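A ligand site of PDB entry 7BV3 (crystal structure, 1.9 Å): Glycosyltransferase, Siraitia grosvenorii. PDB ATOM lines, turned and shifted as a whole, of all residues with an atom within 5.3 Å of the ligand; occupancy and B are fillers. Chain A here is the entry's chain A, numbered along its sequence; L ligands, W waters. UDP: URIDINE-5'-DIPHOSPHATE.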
ATOM      1  N   CYS A 281      13.636   2.731  -2.910  1.00  0.00           N
ATOM      2  CA  CYS A 281      13.802   3.229  -4.271  1.00  0.00           C
ATOM      3  C   CYS A 281      14.388   4.625  -4.239  1.00  0.00           C
ATOM      4  O   CYS A 281      13.985   5.454  -3.404  1.00  0.00           O
ATOM      5  CB  CYS A 281      12.469   3.248  -5.040  1.00  0.00           C
ATOM      6  SG  CYS A 281      12.748   3.355  -6.823  1.00  0.00           S
ATOM      7  N   PHE A 282      15.293   4.908  -5.166  1.00  0.00           N
ATOM      8  CA  PHE A 282      16.129   6.108  -5.029  1.00  0.00           C
ATOM      9  C   PHE A 282      16.097   6.975  -6.288  1.00  0.00           C
ATOM     10  O   PHE A 282      17.113   7.565  -6.680  1.00  0.00           O
ATOM     11  CB  PHE A 282      17.532   5.697  -4.618  1.00  0.00           C
ATOM     12  CG  PHE A 282      17.556   4.839  -3.380  1.00  0.00           C
ATOM     13  CD1 PHE A 282      17.423   5.406  -2.126  1.00  0.00           C
ATOM     14  CD2 PHE A 282      17.605   3.446  -3.482  1.00  0.00           C
ATOM     15  CE1 PHE A 282      17.421   4.603  -0.977  1.00  0.00           C
ATOM     16  CE2 PHE A 282      17.591   2.643  -2.352  1.00  0.00           C
ATOM     17  CZ  PHE A 282      17.511   3.222  -1.099  1.00  0.00           C
ATOM     18  N   GLY A 283      14.916   7.129  -6.888  1.00  0.00           N
ATOM     19  CA  GLY A 283      14.765   8.145  -7.913  1.00  0.00           C
ATOM     20  C   GLY A 283      15.336   7.753  -9.265  1.00  0.00           C
ATOM     21  O   GLY A 283      15.763   6.622  -9.527  1.00  0.00           O
ATOM     22  N   SER A 284      15.371   8.750 -10.153  1.00  0.00           N
ATOM     23  CA  SER A 284      15.808   8.499 -11.510  1.00  0.00           C
ATOM     24  C   SER A 284      17.325   8.555 -11.673  1.00  0.00           C
ATOM     25  O   SER A 284      17.858   7.930 -12.592  1.00  0.00           O
ATOM     26  CB  SER A 284      15.133   9.487 -12.477  1.00  0.00           C
ATOM     27  OG  SER A 284      15.600  10.811 -12.256  1.00  0.00           O
ATOM     28  N   LYS A 285      18.027   9.278 -10.808  1.00  0.00           N
ATOM     29  CA  LYS A 285      19.482   9.348 -10.925  1.00  0.00           C
ATOM     30  C   LYS A 285      20.207   8.697  -9.766  1.00  0.00           C
ATOM     31  O   LYS A 285      21.440   8.668  -9.751  1.00  0.00           O
ATOM     32  CB  LYS A 285      19.937  10.812 -11.059  1.00  0.00           C
ATOM     33  CG  LYS A 285      19.448  11.457 -12.356  1.00  0.00           C
ATOM     34  CD  LYS A 285      20.291  12.666 -12.762  1.00  0.00           C
ATOM     35  CE  LYS A 285      20.282  13.754 -11.707  1.00  0.00           C
ATOM     36  NZ  LYS A 285      19.909  15.067 -12.289  1.00  0.00           N
ATOM     37  N   SER A 310      14.619  -1.772  -5.034  1.00  0.00           N
ATOM     38  CA  SER A 310      15.098  -1.330  -6.332  1.00  0.00           C
ATOM     39  C   SER A 310      16.585  -0.964  -6.224  1.00  0.00           C
ATOM     40  O   SER A 310      16.948  -0.030  -5.509  1.00  0.00           O
ATOM     41  CB  SER A 310      14.268  -0.142  -6.824  1.00  0.00           C
ATOM     42  OG  SER A 310      14.884   0.479  -7.932  1.00  0.00           O
ATOM     43  N   ARG A 312      20.149  -0.214  -8.330  1.00  0.00           N
ATOM     44  CA  ARG A 312      20.812   0.149  -9.601  1.00  0.00           C
ATOM     45  C   ARG A 312      22.259   0.581  -9.336  1.00  0.00           C
ATOM     46  O   ARG A 312      22.522   1.173  -8.282  1.00  0.00           O
ATOM     47  CB  ARG A 312      20.021   1.228 -10.342  1.00  0.00           C
ATOM     48  CG  ARG A 312      18.596   0.805 -10.672  1.00  0.00           C
ATOM     49  CD  ARG A 312      17.712   1.988 -10.995  1.00  0.00           C
ATOM     50  NE  ARG A 312      17.815   2.334 -12.406  1.00  0.00           N
ATOM     51  CZ  ARG A 312      17.705   3.567 -12.880  1.00  0.00           C
ATOM     52  NH1 ARG A 312      17.501   4.579 -12.057  1.00  0.00           N
ATOM     53  NH2 ARG A 312      17.812   3.783 -14.179  1.00  0.00           N
ATOM     54  N   GLY A 349      15.513  -3.851 -10.566  1.00  0.00           N
ATOM     55  CA  GLY A 349      16.078  -2.645 -11.124  1.00  0.00           C
ATOM     56  C   GLY A 349      15.059  -1.521 -11.099  1.00  0.00           C
ATOM     57  O   GLY A 349      14.391  -1.305 -10.088  1.00  0.00           O
ATOM     58  N   TRP A 350      14.938  -0.793 -12.219  1.00  0.00           N
ATOM     59  CA  TRP A 350      13.881   0.197 -12.350  1.00  0.00           C
ATOM     60  C   TRP A 350      12.537  -0.384 -11.922  1.00  0.00           C
ATOM     61  O   TRP A 350      12.144  -1.467 -12.350  1.00  0.00           O
ATOM     62  CB  TRP A 350      13.797   0.687 -13.796  1.00  0.00           C
ATOM     63  CG  TRP A 350      12.751   1.727 -13.982  1.00  0.00           C
ATOM     64  CD1 TRP A 350      11.475   1.541 -14.451  1.00  0.00           C
ATOM     65  CD2 TRP A 350      12.869   3.121 -13.689  1.00  0.00           C
ATOM     66  NE1 TRP A 350      10.809   2.733 -14.472  1.00  0.00           N
ATOM     67  CE2 TRP A 350      11.636   3.727 -14.010  1.00  0.00           C
ATOM     68  CE3 TRP A 350      13.894   3.923 -13.188  1.00  0.00           C
ATOM     69  CZ2 TRP A 350      11.416   5.089 -13.865  1.00  0.00           C
ATOM     70  CZ3 TRP A 350      13.678   5.274 -13.035  1.00  0.00           C
ATOM     71  CH2 TRP A 350      12.443   5.846 -13.366  1.00  0.00           C
ATOM     72  N   ALA A 351      11.819   0.368 -11.064  1.00  0.00           N
ATOM     73  CA  ALA A 351      10.642  -0.146 -10.402  1.00  0.00           C
ATOM     74  C   ALA A 351       9.356   0.548 -10.904  1.00  0.00           C
ATOM     75  O   ALA A 351       9.384   1.708 -11.317  1.00  0.00           O
ATOM     76  CB  ALA A 351      10.745   0.048  -8.882  1.00  0.00           C
ATOM     77  N   PRO A 352       8.236  -0.154 -10.875  1.00  0.00           N
ATOM     78  CA  PRO A 352       6.914   0.497 -11.118  1.00  0.00           C
ATOM     79  C   PRO A 352       6.440   1.167  -9.829  1.00  0.00           C
ATOM     80  O   PRO A 352       5.625   0.660  -9.081  1.00  0.00           O
ATOM     81  CB  PRO A 352       6.038  -0.677 -11.536  1.00  0.00           C
ATOM     82  CG  PRO A 352       6.596  -1.837 -10.788  1.00  0.00           C
ATOM     83  CD  PRO A 352       8.104  -1.611 -10.727  1.00  0.00           C
ATOM     84  N   GLN A 353       6.995   2.354  -9.569  1.00  0.00           N
ATOM     85  CA  GLN A 353       6.963   2.925  -8.225  1.00  0.00           C
ATOM     86  C   GLN A 353       5.537   3.246  -7.768  1.00  0.00           C
ATOM     87  O   GLN A 353       5.140   2.867  -6.663  1.00  0.00           O
ATOM     88  CB  GLN A 353       7.838   4.171  -8.149  1.00  0.00           C
ATOM     89  CG  GLN A 353       7.539   5.031  -6.925  1.00  0.00           C
ATOM     90  CD  GLN A 353       8.722   5.899  -6.528  1.00  0.00           C
ATOM     91  OE1 GLN A 353       9.852   5.505  -6.732  1.00  0.00           O
ATOM     92  NE2 GLN A 353       8.453   7.097  -6.001  1.00  0.00           N
ATOM     93  N   VAL A 354       4.752   3.946  -8.600  1.00  0.00           N
ATOM     94  CA  VAL A 354       3.409   4.331  -8.152  1.00  0.00           C
ATOM     95  C   VAL A 354       2.523   3.104  -7.984  1.00  0.00           C
ATOM     96  O   VAL A 354       1.712   3.040  -7.045  1.00  0.00           O
ATOM     97  CB  VAL A 354       2.759   5.373  -9.081  1.00  0.00           C
ATOM     98  CG1 VAL A 354       3.473   6.716  -8.966  1.00  0.00           C
ATOM     99  CG2 VAL A 354       2.691   4.886 -10.520  1.00  0.00           C
ATOM    100  N   HIS A 368      14.703   8.388  -1.462  1.00  0.00           N
ATOM    101  CA  HIS A 368      15.681   9.472  -1.563  1.00  0.00           C
ATOM    102  C   HIS A 368      15.049  10.866  -1.376  1.00  0.00           C
ATOM    103  O   HIS A 368      15.784  11.854  -1.368  1.00  0.00           O
ATOM    104  CB  HIS A 368      16.441   9.350  -2.899  1.00  0.00           C
ATOM    105  CG  HIS A 368      15.733   9.919  -4.097  1.00  0.00           C
ATOM    106  ND1 HIS A 368      14.397   9.697  -4.361  1.00  0.00           N
ATOM    107  CD2 HIS A 368      16.199  10.649  -5.141  1.00  0.00           C
ATOM    108  CE1 HIS A 368      14.058  10.312  -5.488  1.00  0.00           C
ATOM    109  NE2 HIS A 368      15.141  10.893  -5.986  1.00  0.00           N
ATOM    110  N   CYS A 369      13.723  10.961  -1.227  1.00  0.00           N
ATOM    111  CA  CYS A 369      13.011  12.215  -0.933  1.00  0.00           C
ATOM    112  C   CYS A 369      13.076  13.212  -2.088  1.00  0.00           C
ATOM    113  O   CYS A 369      12.980  14.431  -1.869  1.00  0.00           O
ATOM    114  CB  CYS A 369      13.494  12.871   0.385  1.00  0.00           C
ATOM    115  SG  CYS A 369      12.157  13.639   1.424  1.00  0.00           S
ATOM    116  N   GLY A 370      13.212  12.714  -3.323  1.00  0.00           N
ATOM    117  CA  GLY A 370      12.882  13.544  -4.458  1.00  0.00           C
ATOM    118  C   GLY A 370      11.426  13.947  -4.351  1.00  0.00           C
ATOM    119  O   GLY A 370      10.620  13.253  -3.722  1.00  0.00           O
ATOM    120  N   TRP A 371      11.085  15.110  -4.908  1.00  0.00           N
ATOM    121  CA  TRP A 371       9.790  15.690  -4.573  1.00  0.00           C
ATOM    122  C   TRP A 371       8.632  14.898  -5.164  1.00  0.00           C
ATOM    123  O   TRP A 371       7.565  14.783  -4.540  1.00  0.00           O
ATOM    124  CB  TRP A 371       9.700  17.150  -4.993  1.00  0.00           C
ATOM    125  CG  TRP A 371       8.457  17.829  -4.441  1.00  0.00           C
ATOM    126  CD1 TRP A 371       7.393  18.349  -5.159  1.00  0.00           C
ATOM    127  CD2 TRP A 371       8.118  18.003  -3.057  1.00  0.00           C
ATOM    128  NE1 TRP A 371       6.459  18.855  -4.306  1.00  0.00           N
ATOM    129  CE2 TRP A 371       6.863  18.652  -3.015  1.00  0.00           C
ATOM    130  CE3 TRP A 371       8.759  17.684  -1.851  1.00  0.00           C
ATOM    131  CZ2 TRP A 371       6.233  18.979  -1.800  1.00  0.00           C
ATOM    132  CZ3 TRP A 371       8.137  18.017  -0.647  1.00  0.00           C
ATOM    133  CH2 TRP A 371       6.887  18.656  -0.635  1.00  0.00           C
ATOM    134  N   ASN A 372       8.795  14.341  -6.368  1.00  0.00           N
ATOM    135  CA  ASN A 372       7.682  13.540  -6.919  1.00  0.00           C
ATOM    136  C   ASN A 372       7.479  12.261  -6.103  1.00  0.00           C
ATOM    137  O   ASN A 372       6.334  11.867  -5.849  1.00  0.00           O
ATOM    138  CB  ASN A 372       7.916  13.210  -8.387  1.00  0.00           C
ATOM    139  CG  ASN A 372       7.973  14.470  -9.250  1.00  0.00           C
ATOM    140  OD1 ASN A 372       7.002  15.220  -9.321  1.00  0.00           O
ATOM    141  ND2 ASN A 372       9.133  14.742  -9.846  1.00  0.00           N
ATOM    142  N   SER A 373       8.576  11.628  -5.660  1.00  0.00           N
ATOM    143  CA  SER A 373       8.436  10.460  -4.787  1.00  0.00           C
ATOM    144  C   SER A 373       7.760  10.831  -3.470  1.00  0.00           C
ATOM    145  O   SER A 373       6.986  10.037  -2.924  1.00  0.00           O
ATOM    146  CB  SER A 373       9.802   9.821  -4.513  1.00  0.00           C
ATOM    147  OG  SER A 373      10.341   9.344  -5.720  1.00  0.00           O
ATOM    148  N   THR A 374       8.069  12.008  -2.934  1.00  0.00           N
ATOM    149  CA  THR A 374       7.412  12.460  -1.707  1.00  0.00           C
ATOM    150  C   THR A 374       5.907  12.627  -1.924  1.00  0.00           C
ATOM    151  O   THR A 374       5.099  12.177  -1.112  1.00  0.00           O
ATOM    152  CB  THR A 374       8.034  13.776  -1.261  1.00  0.00           C
ATOM    153  OG1 THR A 374       9.446  13.566  -1.012  1.00  0.00           O
ATOM    154  CG2 THR A 374       7.401  14.296   0.011  1.00  0.00           C
ATOM    155  N   GLU A 376       4.025  11.276  -4.284  1.00  0.00           N
ATOM    156  CA  GLU A 376       3.435   9.967  -4.555  1.00  0.00           C
ATOM    157  C   GLU A 376       3.213   9.174  -3.273  1.00  0.00           C
ATOM    158  O   GLU A 376       2.154   8.565  -3.081  1.00  0.00           O
ATOM    159  CB  GLU A 376       4.330   9.184  -5.522  1.00  0.00           C
ATOM    160  CG  GLU A 376       4.328   9.784  -6.924  1.00  0.00           C
ATOM    161  CD  GLU A 376       5.406   9.198  -7.820  1.00  0.00           C
ATOM    162  OE1 GLU A 376       6.171   8.330  -7.352  1.00  0.00           O
ATOM    163  OE2 GLU A 376       5.502   9.640  -8.984  1.00  0.00           O
ATOM    164  N   TYR A 390      20.958  13.528  -3.681  1.00  0.00           N
ATOM    165  CA  TYR A 390      21.445  14.637  -4.545  1.00  0.00           C
ATOM    166  C   TYR A 390      20.419  15.779  -4.594  1.00  0.00           C
ATOM    167  O   TYR A 390      19.469  15.777  -3.810  1.00  0.00           O
ATOM    168  CB  TYR A 390      21.774  14.120  -5.948  1.00  0.00           C
ATOM    169  CG  TYR A 390      20.687  13.332  -6.625  1.00  0.00           C
ATOM    170  CD1 TYR A 390      20.484  11.990  -6.347  1.00  0.00           C
ATOM    171  CD2 TYR A 390      19.854  13.925  -7.570  1.00  0.00           C
ATOM    172  CE1 TYR A 390      19.486  11.268  -6.970  1.00  0.00           C
ATOM    173  CE2 TYR A 390      18.856  13.211  -8.208  1.00  0.00           C
ATOM    174  CZ  TYR A 390      18.668  11.870  -7.898  1.00  0.00           C
ATOM    175  OH  TYR A 390      17.682  11.155  -8.517  1.00  0.00           O
ATOM    176  N   GLN A 393      17.339  17.103  -2.112  1.00  0.00           N
ATOM    177  CA  GLN A 393      16.763  16.009  -1.292  1.00  0.00           C
ATOM    178  C   GLN A 393      17.070  16.214   0.200  1.00  0.00           C
ATOM    179  O   GLN A 393      16.202  15.902   1.025  1.00  0.00           O
ATOM    180  CB  GLN A 393      17.225  14.637  -1.805  1.00  0.00           C
ATOM    181  CG  GLN A 393      16.516  14.207  -3.069  1.00  0.00           C
ATOM    182  CD  GLN A 393      17.388  13.354  -3.955  1.00  0.00           C
ATOM    183  OE1 GLN A 393      18.189  12.561  -3.477  1.00  0.00           O
ATOM    184  NE2 GLN A 393      17.255  13.533  -5.258  1.00  0.00           N
HETATM  185  N1  UDP L   1      10.520   6.286 -10.513  1.00  0.00           N
HETATM  186  C2  UDP L   1      10.023   5.087 -10.994  1.00  0.00           C
HETATM  187  N3  UDP L   1      10.855   4.006 -10.834  1.00  0.00           N
HETATM  188  C4  UDP L   1      12.110   4.006 -10.252  1.00  0.00           C
HETATM  189  C5  UDP L   1      12.554   5.281  -9.774  1.00  0.00           C
HETATM  190  C6  UDP L   1      11.758   6.363  -9.915  1.00  0.00           C
HETATM  191  O2  UDP L   1       8.928   4.980 -11.524  1.00  0.00           O
HETATM  192  O4  UDP L   1      12.767   2.950 -10.188  1.00  0.00           O
HETATM  193  C1' UDP L   1       9.677   7.475 -10.655  1.00  0.00           C
HETATM  194  C2' UDP L   1       8.979   7.913  -9.370  1.00  0.00           C
HETATM  195  O2' UDP L   1       7.710   7.280  -9.258  1.00  0.00           O
HETATM  196  C3' UDP L   1       8.817   9.419  -9.630  1.00  0.00           C
HETATM  197  C4' UDP L   1      10.118   9.768 -10.356  1.00  0.00           C
HETATM  198  O4' UDP L   1      10.506   8.559 -11.048  1.00  0.00           O
HETATM  199  O3' UDP L   1       7.683   9.696 -10.458  1.00  0.00           O
HETATM  200  C5' UDP L   1      11.248  10.215  -9.460  1.00  0.00           C
HETATM  201  O5' UDP L   1      11.138  11.637  -9.294  1.00  0.00           O
HETATM  202  PA  UDP L   1      11.622  12.347  -7.976  1.00  0.00           P
HETATM  203  O1A UDP L   1      11.191  11.584  -6.737  1.00  0.00           O
HETATM  204  O2A UDP L   1      11.224  13.770  -8.056  1.00  0.00           O
HETATM  205  O3A UDP L   1      13.237  12.228  -8.016  1.00  0.00           O
HETATM  206  PB  UDP L   1      14.264  12.466  -9.200  1.00  0.00           P
HETATM  207  O1B UDP L   1      14.214  11.394 -10.196  1.00  0.00           O
HETATM  208  O2B UDP L   1      15.576  12.645  -8.473  1.00  0.00           O
HETATM  209  O3B UDP L   1      13.867  13.839  -9.761  1.00  0.00           O
HETATM  210  O   HOH W   1      12.570  16.342  -8.521  1.00  0.00           O
HETATM  211  O   HOH W   2      12.465  12.275 -12.385  1.00  0.00           O
HETATM  212  O   HOH W   3       6.088   5.463 -11.109  1.00  0.00           O
HETATM  213  O   HOH W   4      12.075   7.127  -6.556  1.00  0.00           O
HETATM  214  O   HOH W   5      15.254   2.808  -9.650  1.00  0.00           O
HETATM  215  O   HOH W   6      15.333  15.146  -6.810  1.00  0.00           O
HETATM  216  O   HOH W   7       4.976   8.142 -11.612  1.00  0.00           O
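ND2 of Asn 372 is in hydrogen-bond range of O2A of the ligand (2.9 Å). O4 of the ligand is in hydrogen-bond range of N of Ala 351 (2.9 Å). An oxygen (O1A) of the ligand lies within hydrogen-bond range of the side-chain hydroxyl (OG) of Ser 373 (2.6 Å). A ring nitrogen (NE2) of His 368 lies within hydrogen-bond range of an oxygen (O2B) of the ligand. The side-chain carboxylate of Glu 376 sits at hydrogen-bond distance from an oxygen (O3') of the ligand (2.6 Å). An oxygen (O1A) of the ligand lies within hydrogen-bond range of the backbone NH (N) of Ser 373 (2.8 Å). An oxygen (O2B) of the ligand lies within hydrogen-bond range of the side-chain hydroxyl (OH) of Tyr 390 (2.6 Å). The backbone NH of Asn 372 lies within hydrogen-bond range of an oxygen (O2A) of the ligand (3.0 Å). O1B of the ligand lies within hydrogen-bond range of N of Ser 284 (2.9 Å). The backbone NH of Trp 371 sits at hydrogen-bond distance from an oxygen (O2A) of the ligand, 3.4 Å away. An oxygen (O1B) of the ligand sits at hydrogen-bond distance from the side-chain hydroxyl of Ser 284 (2.6 Å). SG of Cys 281 lies within hydrogen-bond range of O4 of the ligand (3.4 Å). An oxygen (O2') of the ligand lies close to the side-chain amide nitrogen (NE2) of Gln 353, 3.3 Å away. The backbone carbonyl oxygen (O) of Ala 351 sits at hydrogen-bond distance from a nitrogen (N3) of the ligand, at 2.8 Å.
The side-chain carboxylate (OE1) of Glu 376 sits at hydrogen-bond distance from the side-chain amide nitrogen (NE2) of Gln 353, at 2.9 Å. The side-chain sulfur (SG) of Cys 281 is in hydrogen-bond range of the side-chain hydroxyl (OG) of Ser 310 (3.8 Å). The backbone carbonyl oxygen (O) of Ser 284 sits at hydrogen-bond distance from the guanidinium group (NH1) of Arg 312. OG of Ser 310 is in hydrogen-bond range of O of Gly 349, 2.8 Å away. The side-chain sulfur of Cys 281 is in hydrogen-bond range of the side-chain amide oxygen of Gln 353, 3.6 Å away. A ring nitrogen (ND1) of His 368 lies close to the backbone NH (N) of Gly 370 (3.4 Å). The backbone NH (N) of Tyr 390 is in hydrogen-bond range of the side-chain amide oxygen (OE1) of Gln 393 (2.9 Å). O of Gly 370 sits at hydrogen-bond distance from OG1 of Thr 374 (3.0 Å).
The backbone carbonyl oxygen of Gly 370 lies close to an oxygen (O1A) of the ligand (3.5 Å). Merely in contact with the ligand: Trp 350 (3.2 Å), Gly 283 (3.5 Å), Gln 393 (3.7 Å) and Ser 310 (3.96 Å). 15 residues have an atom within 4 Å of the ligand: Cys 281, Gly 283, Ser 284, Ser 310, Trp 350, Ala 351, Gln 353, His 368, Gly 370, Trp 371, Asn 372, Ser 373, Glu 376, Tyr 390 and Gln 393.
Water W5 lies within hydrogen-bond range of an oxygen (O4) of the ligand and the side-chain hydroxyl of Ser 310. Water W3 lies within hydrogen-bond range of O2 of the ligand (2.9 Å) and N of Val 354 (3.2 Å). Water W2 lies within hydrogen-bond range of O1B of the ligand and OG of Ser 284. Water W6 lies within hydrogen-bond range of the side-chain amide nitrogen of Gln 393 (3.0 Å) and an oxygen (O2B) of the ligand (3.0 Å). Water W7 bridges OE2 of Glu 376 (3.1 Å) and O3' of the ligand (3.3 Å). Water W4 lies within hydrogen-bond range of OE1 of Gln 353 (2.8 Å), N of Gly 283 (2.9 Å) and OG of Ser 373 (2.9 Å).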
